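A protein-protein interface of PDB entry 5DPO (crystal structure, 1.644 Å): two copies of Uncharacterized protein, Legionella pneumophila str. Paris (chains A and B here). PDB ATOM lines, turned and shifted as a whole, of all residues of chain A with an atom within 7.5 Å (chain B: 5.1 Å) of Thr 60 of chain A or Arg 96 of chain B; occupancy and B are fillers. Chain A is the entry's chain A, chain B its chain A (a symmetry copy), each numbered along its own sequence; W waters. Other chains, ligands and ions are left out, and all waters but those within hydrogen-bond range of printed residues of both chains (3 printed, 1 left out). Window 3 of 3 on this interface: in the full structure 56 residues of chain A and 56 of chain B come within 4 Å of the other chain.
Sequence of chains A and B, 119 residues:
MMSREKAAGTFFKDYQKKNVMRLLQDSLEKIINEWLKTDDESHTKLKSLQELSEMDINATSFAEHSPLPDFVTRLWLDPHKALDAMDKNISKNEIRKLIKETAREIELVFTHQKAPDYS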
ATOM      1  N   MET A  21     -26.400 -12.761  -2.435  1.00  0.00           N
ATOM      2  CA  MET A  21     -25.152 -12.567  -1.705  1.00  0.00           C
ATOM      3  C   MET A  21     -25.127 -11.213  -1.004  1.00  0.00           C
ATOM      4  O   MET A  21     -24.692 -11.113   0.147  1.00  0.00           O
ATOM      5  CB  MET A  21     -23.953 -12.699  -2.650  1.00  0.00           C
ATOM      6  CG  MET A  21     -23.778 -14.100  -3.211  1.00  0.00           C
ATOM      7  SD  MET A  21     -23.423 -15.435  -1.833  1.00  0.00           S
ATOM      8  CE  MET A  21     -21.503 -15.168  -1.616  1.00  0.00           C
ATOM      9  N   LEU A  52     -13.035 -15.477  13.537  1.00  0.00           N
ATOM     10  CA  LEU A  52     -13.918 -15.904  12.455  1.00  0.00           C
ATOM     11  C   LEU A  52     -13.297 -15.593  11.089  1.00  0.00           C
ATOM     12  O   LEU A  52     -13.349 -16.419  10.174  1.00  0.00           O
ATOM     13  CB  LEU A  52     -15.290 -15.237  12.584  1.00  0.00           C
ATOM     14  CG  LEU A  52     -16.338 -15.566  11.520  1.00  0.00           C
ATOM     15  CD1 LEU A  52     -16.656 -17.063  11.503  1.00  0.00           C
ATOM     16  CD2 LEU A  52     -17.597 -14.751  11.771  1.00  0.00           C
ATOM     17  N   SER A  53     -12.677 -14.421  10.961  1.00  0.00           N
ATOM     18  CA  SER A  53     -12.080 -14.021   9.686  1.00  0.00           C
ATOM     19  C   SER A  53     -10.935 -14.943   9.262  1.00  0.00           C
ATOM     20  O   SER A  53     -10.570 -14.974   8.091  1.00  0.00           O
ATOM     21  CB  SER A  53     -11.582 -12.567   9.760  1.00  0.00           C
ATOM     22  OG  SER A  53     -10.378 -12.456  10.513  1.00  0.00           O
ATOM     23  N   MET A  55     -10.908 -18.382  10.126  1.00  0.00           N
ATOM     24  CA  MET A  55     -11.276 -19.757  10.258  1.00  0.00           C
ATOM     25  C   MET A  55     -11.192 -20.530   8.980  1.00  0.00           C
ATOM     26  O   MET A  55     -11.420 -19.994   7.957  1.00  0.00           O
ATOM     27  CB  MET A  55     -12.711 -19.916  10.694  1.00  0.00           C
ATOM     28  CG  MET A  55     -13.154 -19.979  12.104  1.00  0.00           C
ATOM     29  SD  MET A  55     -12.040 -20.861  13.484  1.00  0.00           S
ATOM     30  CE  MET A  55     -12.721 -19.743  15.022  1.00  0.00           C
ATOM     31  N   ASP A  56     -10.813 -21.786   9.093  1.00  0.00           N
ATOM     32  CA  ASP A  56     -10.794 -22.711   7.966  1.00  0.00           C
ATOM     33  C   ASP A  56     -12.234 -22.951   7.507  1.00  0.00           C
ATOM     34  O   ASP A  56     -13.103 -23.241   8.327  1.00  0.00           O
ATOM     35  CB  ASP A  56     -10.110 -24.019   8.397  1.00  0.00           C
ATOM     36  CG  ASP A  56      -9.838 -24.966   7.244  1.00  0.00           C
ATOM     37  OD1 ASP A  56     -10.744 -25.208   6.425  1.00  0.00           O
ATOM     38  OD2 ASP A  56      -8.703 -25.489   7.175  1.00  0.00           O
ATOM     39  N   ILE A  57     -12.507 -22.829   6.209  1.00  0.00           N
ATOM     40  CA  ILE A  57     -13.896 -22.967   5.767  1.00  0.00           C
ATOM     41  C   ILE A  57     -14.388 -24.413   5.833  1.00  0.00           C
ATOM     42  O   ILE A  57     -15.565 -24.674   5.580  1.00  0.00           O
ATOM     43  CB  ILE A  57     -14.115 -22.429   4.332  1.00  0.00           C
ATOM     44  CG1 ILE A  57     -13.241 -23.167   3.319  1.00  0.00           C
ATOM     45  CG2 ILE A  57     -13.887 -20.917   4.283  1.00  0.00           C
ATOM     46  CD1 ILE A  57     -13.536 -22.771   1.886  1.00  0.00           C
ATOM     47  N   ASN A  58     -13.502 -25.345   6.179  1.00  0.00           N
ATOM     48  CA  ASN A  58     -13.920 -26.727   6.419  1.00  0.00           C
ATOM     49  C   ASN A  58     -14.255 -27.001   7.877  1.00  0.00           C
ATOM     50  O   ASN A  58     -14.690 -28.099   8.223  1.00  0.00           O
ATOM     51  CB  ASN A  58     -12.838 -27.719   5.980  1.00  0.00           C
ATOM     52  CG  ASN A  58     -12.601 -27.704   4.492  1.00  0.00           C
ATOM     53  OD1 ASN A  58     -11.459 -27.647   4.035  1.00  0.00           O
ATOM     54  ND2 ASN A  58     -13.677 -27.752   3.722  1.00  0.00           N
ATOM     55  N   ALA A  59     -14.039 -26.008   8.732  1.00  0.00           N
ATOM     56  CA  ALA A  59     -14.241 -26.182  10.165  1.00  0.00           C
ATOM     57  C   ALA A  59     -15.660 -25.817  10.590  1.00  0.00           C
ATOM     58  O   ALA A  59     -16.254 -24.886  10.042  1.00  0.00           O
ATOM     59  CB  ALA A  59     -13.236 -25.347  10.934  1.00  0.00           C
ATOM     60  N   THR A  60     -16.194 -26.535  11.576  1.00  0.00           N
ATOM     61  CA  THR A  60     -17.526 -26.234  12.101  1.00  0.00           C
ATOM     62  C   THR A  60     -17.625 -26.281  13.627  1.00  0.00           C
ATOM     63  O   THR A  60     -18.564 -25.736  14.200  1.00  0.00           O
ATOM     64  CB  THR A  60     -18.594 -27.204  11.528  1.00  0.00           C
ATOM     65  OG1 THR A  60     -18.188 -28.561  11.752  1.00  0.00           O
ATOM     66  CG2 THR A  60     -18.796 -26.975  10.037  1.00  0.00           C
ATOM     67  N   SER A  61     -16.659 -26.911  14.290  1.00  0.00           N
ATOM     68  CA  SER A  61     -16.736 -27.122  15.732  1.00  0.00           C
ATOM     69  C   SER A  61     -16.815 -25.817  16.528  1.00  0.00           C
ATOM     70  O   SER A  61     -17.513 -25.741  17.540  1.00  0.00           O
ATOM     71  CB  SER A  61     -15.538 -27.947  16.209  1.00  0.00           C
ATOM     72  OG  SER A  61     -15.636 -28.225  17.594  1.00  0.00           O
ATOM     73  N   PHE A  62     -16.101 -24.791  16.072  1.00  0.00           N
ATOM     74  CA  PHE A  62     -16.065 -23.518  16.780  1.00  0.00           C
ATOM     75  C   PHE A  62     -17.455 -22.902  16.909  1.00  0.00           C
ATOM     76  O   PHE A  62     -17.715 -22.113  17.813  1.00  0.00           O
ATOM     77  CB  PHE A  62     -15.136 -22.533  16.064  1.00  0.00           C
ATOM     78  CG  PHE A  62     -15.709 -21.991  14.784  1.00  0.00           C
ATOM     79  CD1 PHE A  62     -15.583 -22.699  13.600  1.00  0.00           C
ATOM     80  CD2 PHE A  62     -16.385 -20.779  14.769  1.00  0.00           C
ATOM     81  CE1 PHE A  62     -16.117 -22.211  12.421  1.00  0.00           C
ATOM     82  CE2 PHE A  62     -16.934 -20.291  13.603  1.00  0.00           C
ATOM     83  CZ  PHE A  62     -16.797 -21.006  12.419  1.00  0.00           C
ATOM     84  N   ALA A  63     -18.341 -23.262  15.988  1.00  0.00           N
ATOM     85  CA  ALA A  63     -19.621 -22.577  15.862  1.00  0.00           C
ATOM     86  C   ALA A  63     -20.680 -23.104  16.824  1.00  0.00           C
ATOM     87  O   ALA A  63     -21.732 -22.487  16.982  1.00  0.00           O
ATOM     88  CB  ALA A  63     -20.121 -22.677  14.430  1.00  0.00           C
ATOM     89  N   GLU A  64     -20.397 -24.214  17.485  1.00  0.00           N
ATOM     90  CA  GLU A  64     -21.390 -24.748  18.391  1.00  0.00           C
ATOM     91  C   GLU A  64     -21.417 -24.079  19.702  1.00  0.00           C
ATOM     92  O   GLU A  64     -22.464 -23.904  20.246  1.00  0.00           O
ATOM     93  CB  GLU A  64     -21.209 -26.202  18.664  1.00  0.00           C
ATOM     94  CG  GLU A  64     -20.528 -26.938  17.579  1.00  0.00           C
ATOM     95  CD  GLU A  64     -21.269 -27.024  16.267  1.00  0.00           C
ATOM     96  OE1 GLU A  64     -22.526 -27.121  16.194  1.00  0.00           O
ATOM     97  OE2 GLU A  64     -20.583 -27.046  15.272  1.00  0.00           O
ATOM     98  N   HIS A  65     -20.271 -23.716  20.224  1.00  0.00           N
ATOM     99  CA  HIS A  65     -20.182 -22.940  21.453  1.00  0.00           C
ATOM    100  C   HIS A  65     -19.408 -21.656  21.189  1.00  0.00           C
ATOM    101  O   HIS A  65     -18.193 -21.607  21.371  1.00  0.00           O
ATOM    102  CB  HIS A  65     -19.510 -23.755  22.558  1.00  0.00           C
ATOM    103  CG  HIS A  65     -19.508 -23.077  23.893  1.00  0.00           C
ATOM    104  ND1 HIS A  65     -20.653 -22.576  24.475  1.00  0.00           N
ATOM    105  CD2 HIS A  65     -18.501 -22.819  24.762  1.00  0.00           C
ATOM    106  CE1 HIS A  65     -20.352 -22.038  25.643  1.00  0.00           C
ATOM    107  NE2 HIS A  65     -19.052 -22.172  25.841  1.00  0.00           N
ATOM    108  N   THR A  73     -23.530 -17.975  13.049  1.00  0.00           N
ATOM    109  CA  THR A  73     -23.135 -19.373  13.139  1.00  0.00           C
ATOM    110  C   THR A  73     -24.118 -20.284  12.408  1.00  0.00           C
ATOM    111  O   THR A  73     -23.710 -21.306  11.875  1.00  0.00           O
ATOM    112  CB  THR A  73     -22.970 -19.837  14.599  1.00  0.00           C
ATOM    113  OG1 THR A  73     -24.103 -19.434  15.380  1.00  0.00           O
ATOM    114  CG2 THR A  73     -21.708 -19.226  15.192  1.00  0.00           C
ATOM    115  N   ARG A  74     -25.394 -19.908  12.355  1.00  0.00           N
ATOM    116  CA  ARG A  74     -26.361 -20.694  11.593  1.00  0.00           C
ATOM    117  C   ARG A  74     -26.052 -20.622  10.107  1.00  0.00           C
ATOM    118  O   ARG A  74     -26.096 -21.636   9.408  1.00  0.00           O
ATOM    119  CB  ARG A  74     -27.796 -20.229  11.851  1.00  0.00           C
ATOM    120  CG  ARG A  74     -28.372 -20.702  13.176  1.00  0.00           C
ATOM    121  CD  ARG A  74     -29.879 -20.459  13.249  1.00  0.00           C
ATOM    122  NE  ARG A  74     -30.214 -19.039  13.302  1.00  0.00           N
ATOM    123  CZ  ARG A  74     -30.696 -18.340  12.278  1.00  0.00           C
ATOM    124  NH1 ARG A  74     -30.906 -18.928  11.107  1.00  0.00           N
ATOM    125  NH2 ARG A  74     -30.970 -17.050  12.426  1.00  0.00           N
ATOM    126  N   LEU A  75     -25.736 -19.424   9.622  1.00  0.00           N
ATOM    127  CA  LEU A  75     -25.400 -19.253   8.212  1.00  0.00           C
ATOM    128  C   LEU A  75     -24.131 -20.021   7.852  1.00  0.00           C
ATOM    129  O   LEU A  75     -24.050 -20.622   6.790  1.00  0.00           O
ATOM    130  CB  LEU A  75     -25.236 -17.773   7.870  1.00  0.00           C
ATOM    131  CG  LEU A  75     -25.008 -17.442   6.392  1.00  0.00           C
ATOM    132  CD1 LEU A  75     -26.224 -17.799   5.536  1.00  0.00           C
ATOM    133  CD2 LEU A  75     -24.622 -15.975   6.225  1.00  0.00           C
ATOM    134  N   TRP A  76     -23.145 -19.999   8.740  1.00  0.00           N
ATOM    135  CA  TRP A  76     -21.919 -20.772   8.533  1.00  0.00           C
ATOM    136  C   TRP A  76     -22.191 -22.280   8.488  1.00  0.00           C
ATOM    137  O   TRP A  76     -21.753 -22.981   7.572  1.00  0.00           O
ATOM    138  CB  TRP A  76     -20.910 -20.454   9.646  1.00  0.00           C
ATOM    139  CG  TRP A  76     -19.607 -21.200   9.514  1.00  0.00           C
ATOM    140  CD1 TRP A  76     -19.371 -22.493   9.865  1.00  0.00           C
ATOM    141  CD2 TRP A  76     -18.363 -20.693   8.997  1.00  0.00           C
ATOM    142  NE1 TRP A  76     -18.064 -22.830   9.592  1.00  0.00           N
ATOM    143  CE2 TRP A  76     -17.426 -21.743   9.066  1.00  0.00           C
ATOM    144  CE3 TRP A  76     -17.955 -19.457   8.490  1.00  0.00           C
ATOM    145  CZ2 TRP A  76     -16.107 -21.598   8.638  1.00  0.00           C
ATOM    146  CZ3 TRP A  76     -16.635 -19.315   8.066  1.00  0.00           C
ATOM    147  CH2 TRP A  76     -15.732 -20.376   8.151  1.00  0.00           C
ATOM    148  N   LEU A  77     -22.922 -22.772   9.485  1.00  0.00           N
ATOM    149  CA  LEU A  77     -23.119 -24.207   9.650  1.00  0.00           C
ATOM    150  C   LEU A  77     -23.943 -24.822   8.524  1.00  0.00           C
ATOM    151  O   LEU A  77     -23.652 -25.927   8.071  1.00  0.00           O
ATOM    152  CB  LEU A  77     -23.778 -24.497  10.998  1.00  0.00           C
ATOM    153  CG  LEU A  77     -22.827 -24.351  12.187  1.00  0.00           C
ATOM    154  CD1 LEU A  77     -23.587 -24.384  13.504  1.00  0.00           C
ATOM    155  CD2 LEU A  77     -21.764 -25.439  12.139  1.00  0.00           C
ATOM    156  N   ASP A  78     -24.968 -24.111   8.071  1.00  0.00           N
ATOM    157  CA  ASP A  78     -25.863 -24.649   7.054  1.00  0.00           C
ATOM    158  C   ASP A  78     -26.505 -23.504   6.284  1.00  0.00           C
ATOM    159  O   ASP A  78     -27.617 -23.097   6.604  1.00  0.00           O
ATOM    160  CB  ASP A  78     -26.927 -25.534   7.707  1.00  0.00           C
ATOM    161  CG  ASP A  78     -27.651 -26.430   6.709  1.00  0.00           C
ATOM    162  OD1 ASP A  78     -27.782 -26.055   5.525  1.00  0.00           O
ATOM    163  OD2 ASP A  78     -28.107 -27.514   7.127  1.00  0.00           O
ATOM    164  N   PRO A  79     -25.795 -22.973   5.277  1.00  0.00           N
ATOM    165  CA  PRO A  79     -26.259 -21.794   4.537  1.00  0.00           C
ATOM    166  C   PRO A  79     -27.636 -21.987   3.914  1.00  0.00           C
ATOM    167  O   PRO A  79     -28.479 -21.094   4.009  1.00  0.00           O
ATOM    168  CB  PRO A  79     -25.188 -21.616   3.453  1.00  0.00           C
ATOM    169  CG  PRO A  79     -23.968 -22.241   4.022  1.00  0.00           C
ATOM    170  CD  PRO A  79     -24.450 -23.399   4.850  1.00  0.00           C
ATOM    171  N   LYS B  92     -21.654 -23.782  -0.193  1.00  0.00           N
ATOM    172  CA  LYS B  92     -21.298 -23.616   1.199  1.00  0.00           C
ATOM    173  C   LYS B  92     -19.958 -22.883   1.301  1.00  0.00           C
ATOM    174  O   LYS B  92     -19.801 -21.979   2.128  1.00  0.00           O
ATOM    175  CB  LYS B  92     -21.249 -24.980   1.892  1.00  0.00           C
ATOM    176  CG  LYS B  92     -20.747 -24.963   3.315  1.00  0.00           C
ATOM    177  CD  LYS B  92     -20.800 -26.367   3.912  1.00  0.00           C
ATOM    178  CE  LYS B  92     -22.232 -26.826   4.116  1.00  0.00           C
ATOM    179  NZ  LYS B  92     -22.299 -28.074   4.924  1.00  0.00           N
ATOM    180  N   ASN B  93     -19.010 -23.237   0.434  1.00  0.00           N
ATOM    181  CA  ASN B  93     -17.706 -22.565   0.395  1.00  0.00           C
ATOM    182  C   ASN B  93     -17.826 -21.070   0.120  1.00  0.00           C
ATOM    183  O   ASN B  93     -17.122 -20.266   0.727  1.00  0.00           O
ATOM    184  CB  ASN B  93     -16.796 -23.179  -0.673  1.00  0.00           C
ATOM    185  CG  ASN B  93     -16.124 -24.461  -0.224  1.00  0.00           C
ATOM    186  OD1 ASN B  93     -16.130 -24.809   0.953  1.00  0.00           O
ATOM    187  ND2 ASN B  93     -15.527 -25.169  -1.177  1.00  0.00           N
ATOM    188  N   GLU B  94     -18.698 -20.703  -0.813  1.00  0.00           N
ATOM    189  CA  GLU B  94     -18.884 -19.297  -1.161  1.00  0.00           C
ATOM    190  C   GLU B  94     -19.435 -18.501   0.014  1.00  0.00           C
ATOM    191  O   GLU B  94     -19.004 -17.380   0.266  1.00  0.00           O
ATOM    192  CB  GLU B  94     -19.824 -19.152  -2.360  1.00  0.00           C
ATOM    193  CG  GLU B  94     -19.176 -19.485  -3.687  1.00  0.00           C
ATOM    194  CD  GLU B  94     -20.143 -19.372  -4.845  1.00  0.00           C
ATOM    195  OE1 GLU B  94     -21.311 -19.783  -4.680  1.00  0.00           O
ATOM    196  OE2 GLU B  94     -19.733 -18.878  -5.917  1.00  0.00           O
ATOM    197  N   ILE B  95     -20.400 -19.077   0.723  1.00  0.00           N
ATOM    198  CA  ILE B  95     -20.997 -18.396   1.873  1.00  0.00           C
ATOM    199  C   ILE B  95     -19.995 -18.251   3.014  1.00  0.00           C
ATOM    200  O   ILE B  95     -19.905 -17.194   3.632  1.00  0.00           O
ATOM    201  CB  ILE B  95     -22.246 -19.142   2.379  1.00  0.00           C
ATOM    202  CG1 ILE B  95     -23.338 -19.087   1.319  1.00  0.00           C
ATOM    203  CG2 ILE B  95     -22.759 -18.520   3.680  1.00  0.00           C
ATOM    204  CD1 ILE B  95     -23.685 -17.687   0.915  1.00  0.00           C
ATOM    205  N   ARG B  96     -19.238 -19.303   3.299  1.00  0.00           N
ATOM    206  CA  ARG B  96     -18.281 -19.202   4.393  1.00  0.00           C
ATOM    207  C   ARG B  96     -17.183 -18.198   4.044  1.00  0.00           C
ATOM    208  O   ARG B  96     -16.728 -17.457   4.913  1.00  0.00           O
ATOM    209  CB  ARG B  96     -17.700 -20.574   4.750  1.00  0.00           C
ATOM    210  CG  ARG B  96     -18.771 -21.471   5.350  1.00  0.00           C
ATOM    211  CD  ARG B  96     -18.279 -22.855   5.704  1.00  0.00           C
ATOM    212  NE  ARG B  96     -19.366 -23.615   6.310  1.00  0.00           N
ATOM    213  CZ  ARG B  96     -19.300 -24.906   6.618  1.00  0.00           C
ATOM    214  NH1 ARG B  96     -18.193 -25.596   6.371  1.00  0.00           N
ATOM    215  NH2 ARG B  96     -20.351 -25.513   7.157  1.00  0.00           N
ATOM    216  N   LYS B  97     -16.783 -18.147   2.775  1.00  0.00           N
ATOM    217  CA  LYS B  97     -15.844 -17.116   2.338  1.00  0.00           C
ATOM    218  C   LYS B  97     -16.428 -15.717   2.520  1.00  0.00           C
ATOM    219  O   LYS B  97     -15.730 -14.804   2.963  1.00  0.00           O
ATOM    220  CB  LYS B  97     -15.432 -17.330   0.875  1.00  0.00           C
ATOM    221  CG  LYS B  97     -14.437 -18.466   0.686  1.00  0.00           C
ATOM    222  CD  LYS B  97     -14.055 -18.643  -0.774  1.00  0.00           C
ATOM    223  CE  LYS B  97     -13.202 -19.884  -0.962  1.00  0.00           C
ATOM    224  NZ  LYS B  97     -11.968 -19.822  -0.131  1.00  0.00           N
ATOM    225  N   LEU B  98     -17.703 -15.545   2.179  1.00  0.00           N
ATOM    226  CA  LEU B  98     -18.373 -14.261   2.368  1.00  0.00           C
ATOM    227  C   LEU B  98     -18.386 -13.859   3.839  1.00  0.00           C
ATOM    228  O   LEU B  98     -18.143 -12.699   4.184  1.00  0.00           O
ATOM    229  CB  LEU B  98     -19.807 -14.313   1.829  1.00  0.00           C
ATOM    230  CG  LEU B  98     -20.681 -13.095   2.139  1.00  0.00           C
ATOM    231  CD1 LEU B  98     -20.176 -11.878   1.385  1.00  0.00           C
ATOM    232  CD2 LEU B  98     -22.141 -13.378   1.786  1.00  0.00           C
ATOM    233  N   ILE B  99     -18.672 -14.819   4.709  1.00  0.00           N
ATOM    234  CA  ILE B  99     -18.663 -14.556   6.145  1.00  0.00           C
ATOM    235  C   ILE B  99     -17.278 -14.112   6.628  1.00  0.00           C
ATOM    236  O   ILE B  99     -17.167 -13.142   7.362  1.00  0.00           O
ATOM    237  CB  ILE B  99     -19.122 -15.789   6.938  1.00  0.00           C
ATOM    238  CG1 ILE B  99     -20.614 -16.049   6.677  1.00  0.00           C
ATOM    239  CG2 ILE B  99     -18.895 -15.587   8.418  1.00  0.00           C
ATOM    240  CD1 ILE B  99     -21.082 -17.406   7.164  1.00  0.00           C
ATOM    241  N   LYS B 100     -16.226 -14.808   6.208  1.00  0.00           N
ATOM    242  CA  LYS B 100     -14.867 -14.413   6.592  1.00  0.00           C
ATOM    243  C   LYS B 100     -14.508 -13.030   6.059  1.00  0.00           C
ATOM    244  O   LYS B 100     -13.930 -12.207   6.776  1.00  0.00           O
ATOM    245  CB  LYS B 100     -13.838 -15.427   6.095  1.00  0.00           C
ATOM    246  CG  LYS B 100     -13.961 -16.800   6.736  1.00  0.00           C
ATOM    247  CD  LYS B 100     -13.037 -17.813   6.066  1.00  0.00           C
ATOM    248  CE  LYS B 100     -11.578 -17.406   6.226  1.00  0.00           C
ATOM    249  NZ  LYS B 100     -10.674 -18.447   5.678  1.00  0.00           N
ATOM    250  N   GLU B 101     -14.849 -12.780   4.797  1.00  0.00           N
ATOM    251  CA  GLU B 101     -14.553 -11.490   4.169  1.00  0.00           C
ATOM    252  C   GLU B 101     -15.276 -10.349   4.871  1.00  0.00           C
ATOM    253  O   GLU B 101     -14.716  -9.273   5.078  1.00  0.00           O
ATOM    254  CB  GLU B 101     -14.932 -11.517   2.685  1.00  0.00           C
ATOM    255  CG  GLU B 101     -13.985 -12.347   1.831  1.00  0.00           C
ATOM    256  CD  GLU B 101     -14.541 -12.620   0.443  1.00  0.00           C
ATOM    257  OE1 GLU B 101     -15.675 -12.171   0.154  1.00  0.00           O
ATOM    258  OE2 GLU B 101     -13.850 -13.290  -0.354  1.00  0.00           O
HETATM  259  O   HOH W   1     -13.609 -26.178   1.463  1.00  0.00           O
HETATM  260  O   HOH W   2     -10.175 -21.697   4.567  1.00  0.00           O
HETATM  261  O   HOH W   3     -10.563 -12.748   6.126  1.00  0.00           O
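Among the printed residues, pairs that only touch across the chains: Ser 53 of chain A with Lys 100 of chain B (3.2 Å), Ile 57 of chain A with Asn 93 of chain B (3.4 Å), Leu 52 of chain A with Lys 100 of chain B (3.5 Å), Met 21 of chain A with Ile 95 of chain B (3.6 Å), Thr 60 of chain A with Arg 96 of chain B (3.6 Å), Trp 76 of chain A with Ile 99 of chain B (3.7 Å), Ile 57 of chain A with Lys 100 of chain B (3.7 Å), Leu 75 of chain A with Ile 95 of chain B (3.7 Å), Leu 52 of chain A with Ile 99 of chain B (3.7 Å), Met 21 of chain A with Leu 98 of chain B (3.8 Å), Pro 79 of chain A with Ile 95 of chain B (3.8 Å), Met 21 of chain A with Glu 94 of chain B (3.8 Å), Ile 57 of chain A with Lys 97 of chain B (3.9 Å), Trp 76 of chain A with Lys 100 of chain B (3.9 Å) and Leu 75 of chain A with Ile 99 of chain B (3.9 Å).
The backbone carbonyl oxygen (O) of Trp 76 of chain A sits at hydrogen-bond distance from the guanidinium group (NE) of Arg 96 of chain B (2.8 Å). O of Leu 77 of chain A lies within hydrogen-bond range of NH2 of Arg 96 of chain B (3.5 Å). The backbone carbonyl oxygen (O) of Ile 57 of chain A is in hydrogen-bond range of the guanidinium group (NH1) of Arg 96 of chain B (2.9 Å). The backbone carbonyl oxygen of Met 55 of chain A lies within hydrogen-bond range of the side-chain amino group of Lys 100 of chain B (2.9 Å).
No position is printed for both chains. Of the 19 pairs that touch across the chains among the printed residues, none has its exchanged pair printed and touching as well.
Thr 60 of chain A touches just one residue of chain B: Arg 96. Of the printed residues of chain B, Trp 76 of chain A touches Arg 96, Ile 99 and Lys 100. Printed residues of chain B within 4 Å of Met 21 of chain A: Glu 94 (3.8 Å), Ile 95 (3.6 Å) and Leu 98 (3.8 Å). Of the printed residues of chain A, Glu 94 of chain B touches Met 21. The nearest printed residue of chain A that does not touch Leu 98 of chain B is Leu 75 of chain A (5.7 Å).
Water W1 lies within hydrogen-bond range of the side-chain amide nitrogen of Asn 58 of chain A (2.8 Å) and the side-chain amide oxygen of Asn 93 of chain B (2.9 Å). Water W3 lies within hydrogen-bond range of O of Ser 53 of chain A (3.0 Å) and O of Lys 100 of chain B (3.5 Å). Water W2 lies within hydrogen-bond range of N of Ile 57 of chain A (3.1 Å) and NZ of Lys 100 of chain B (3.5 Å).
The backbone carbonyl oxygen (O) of Ala 59 of chain A is in hydrogen-bond range of the indole nitrogen (NE1) of Trp 76 of chain A, at 2.8 Å. The backbone carbonyl oxygen (O) of Thr 60 of chain A lies close to the side-chain carboxylate (OE2) of Glu 64 of chain A.
Of the 21 printed residues of chain A, 10 touch a printed residue of chain B. Printed residues of chain B that touch a printed residue of chain A: Asn 93, Glu 94, Ile 95, Arg 96, Lys 97, Leu 98, Ile 99 and Lys 100. Hydrophobic or aromatic side chains of chain B that line the printed part of chain A: Ile 95, Leu 98 and Ile 99.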
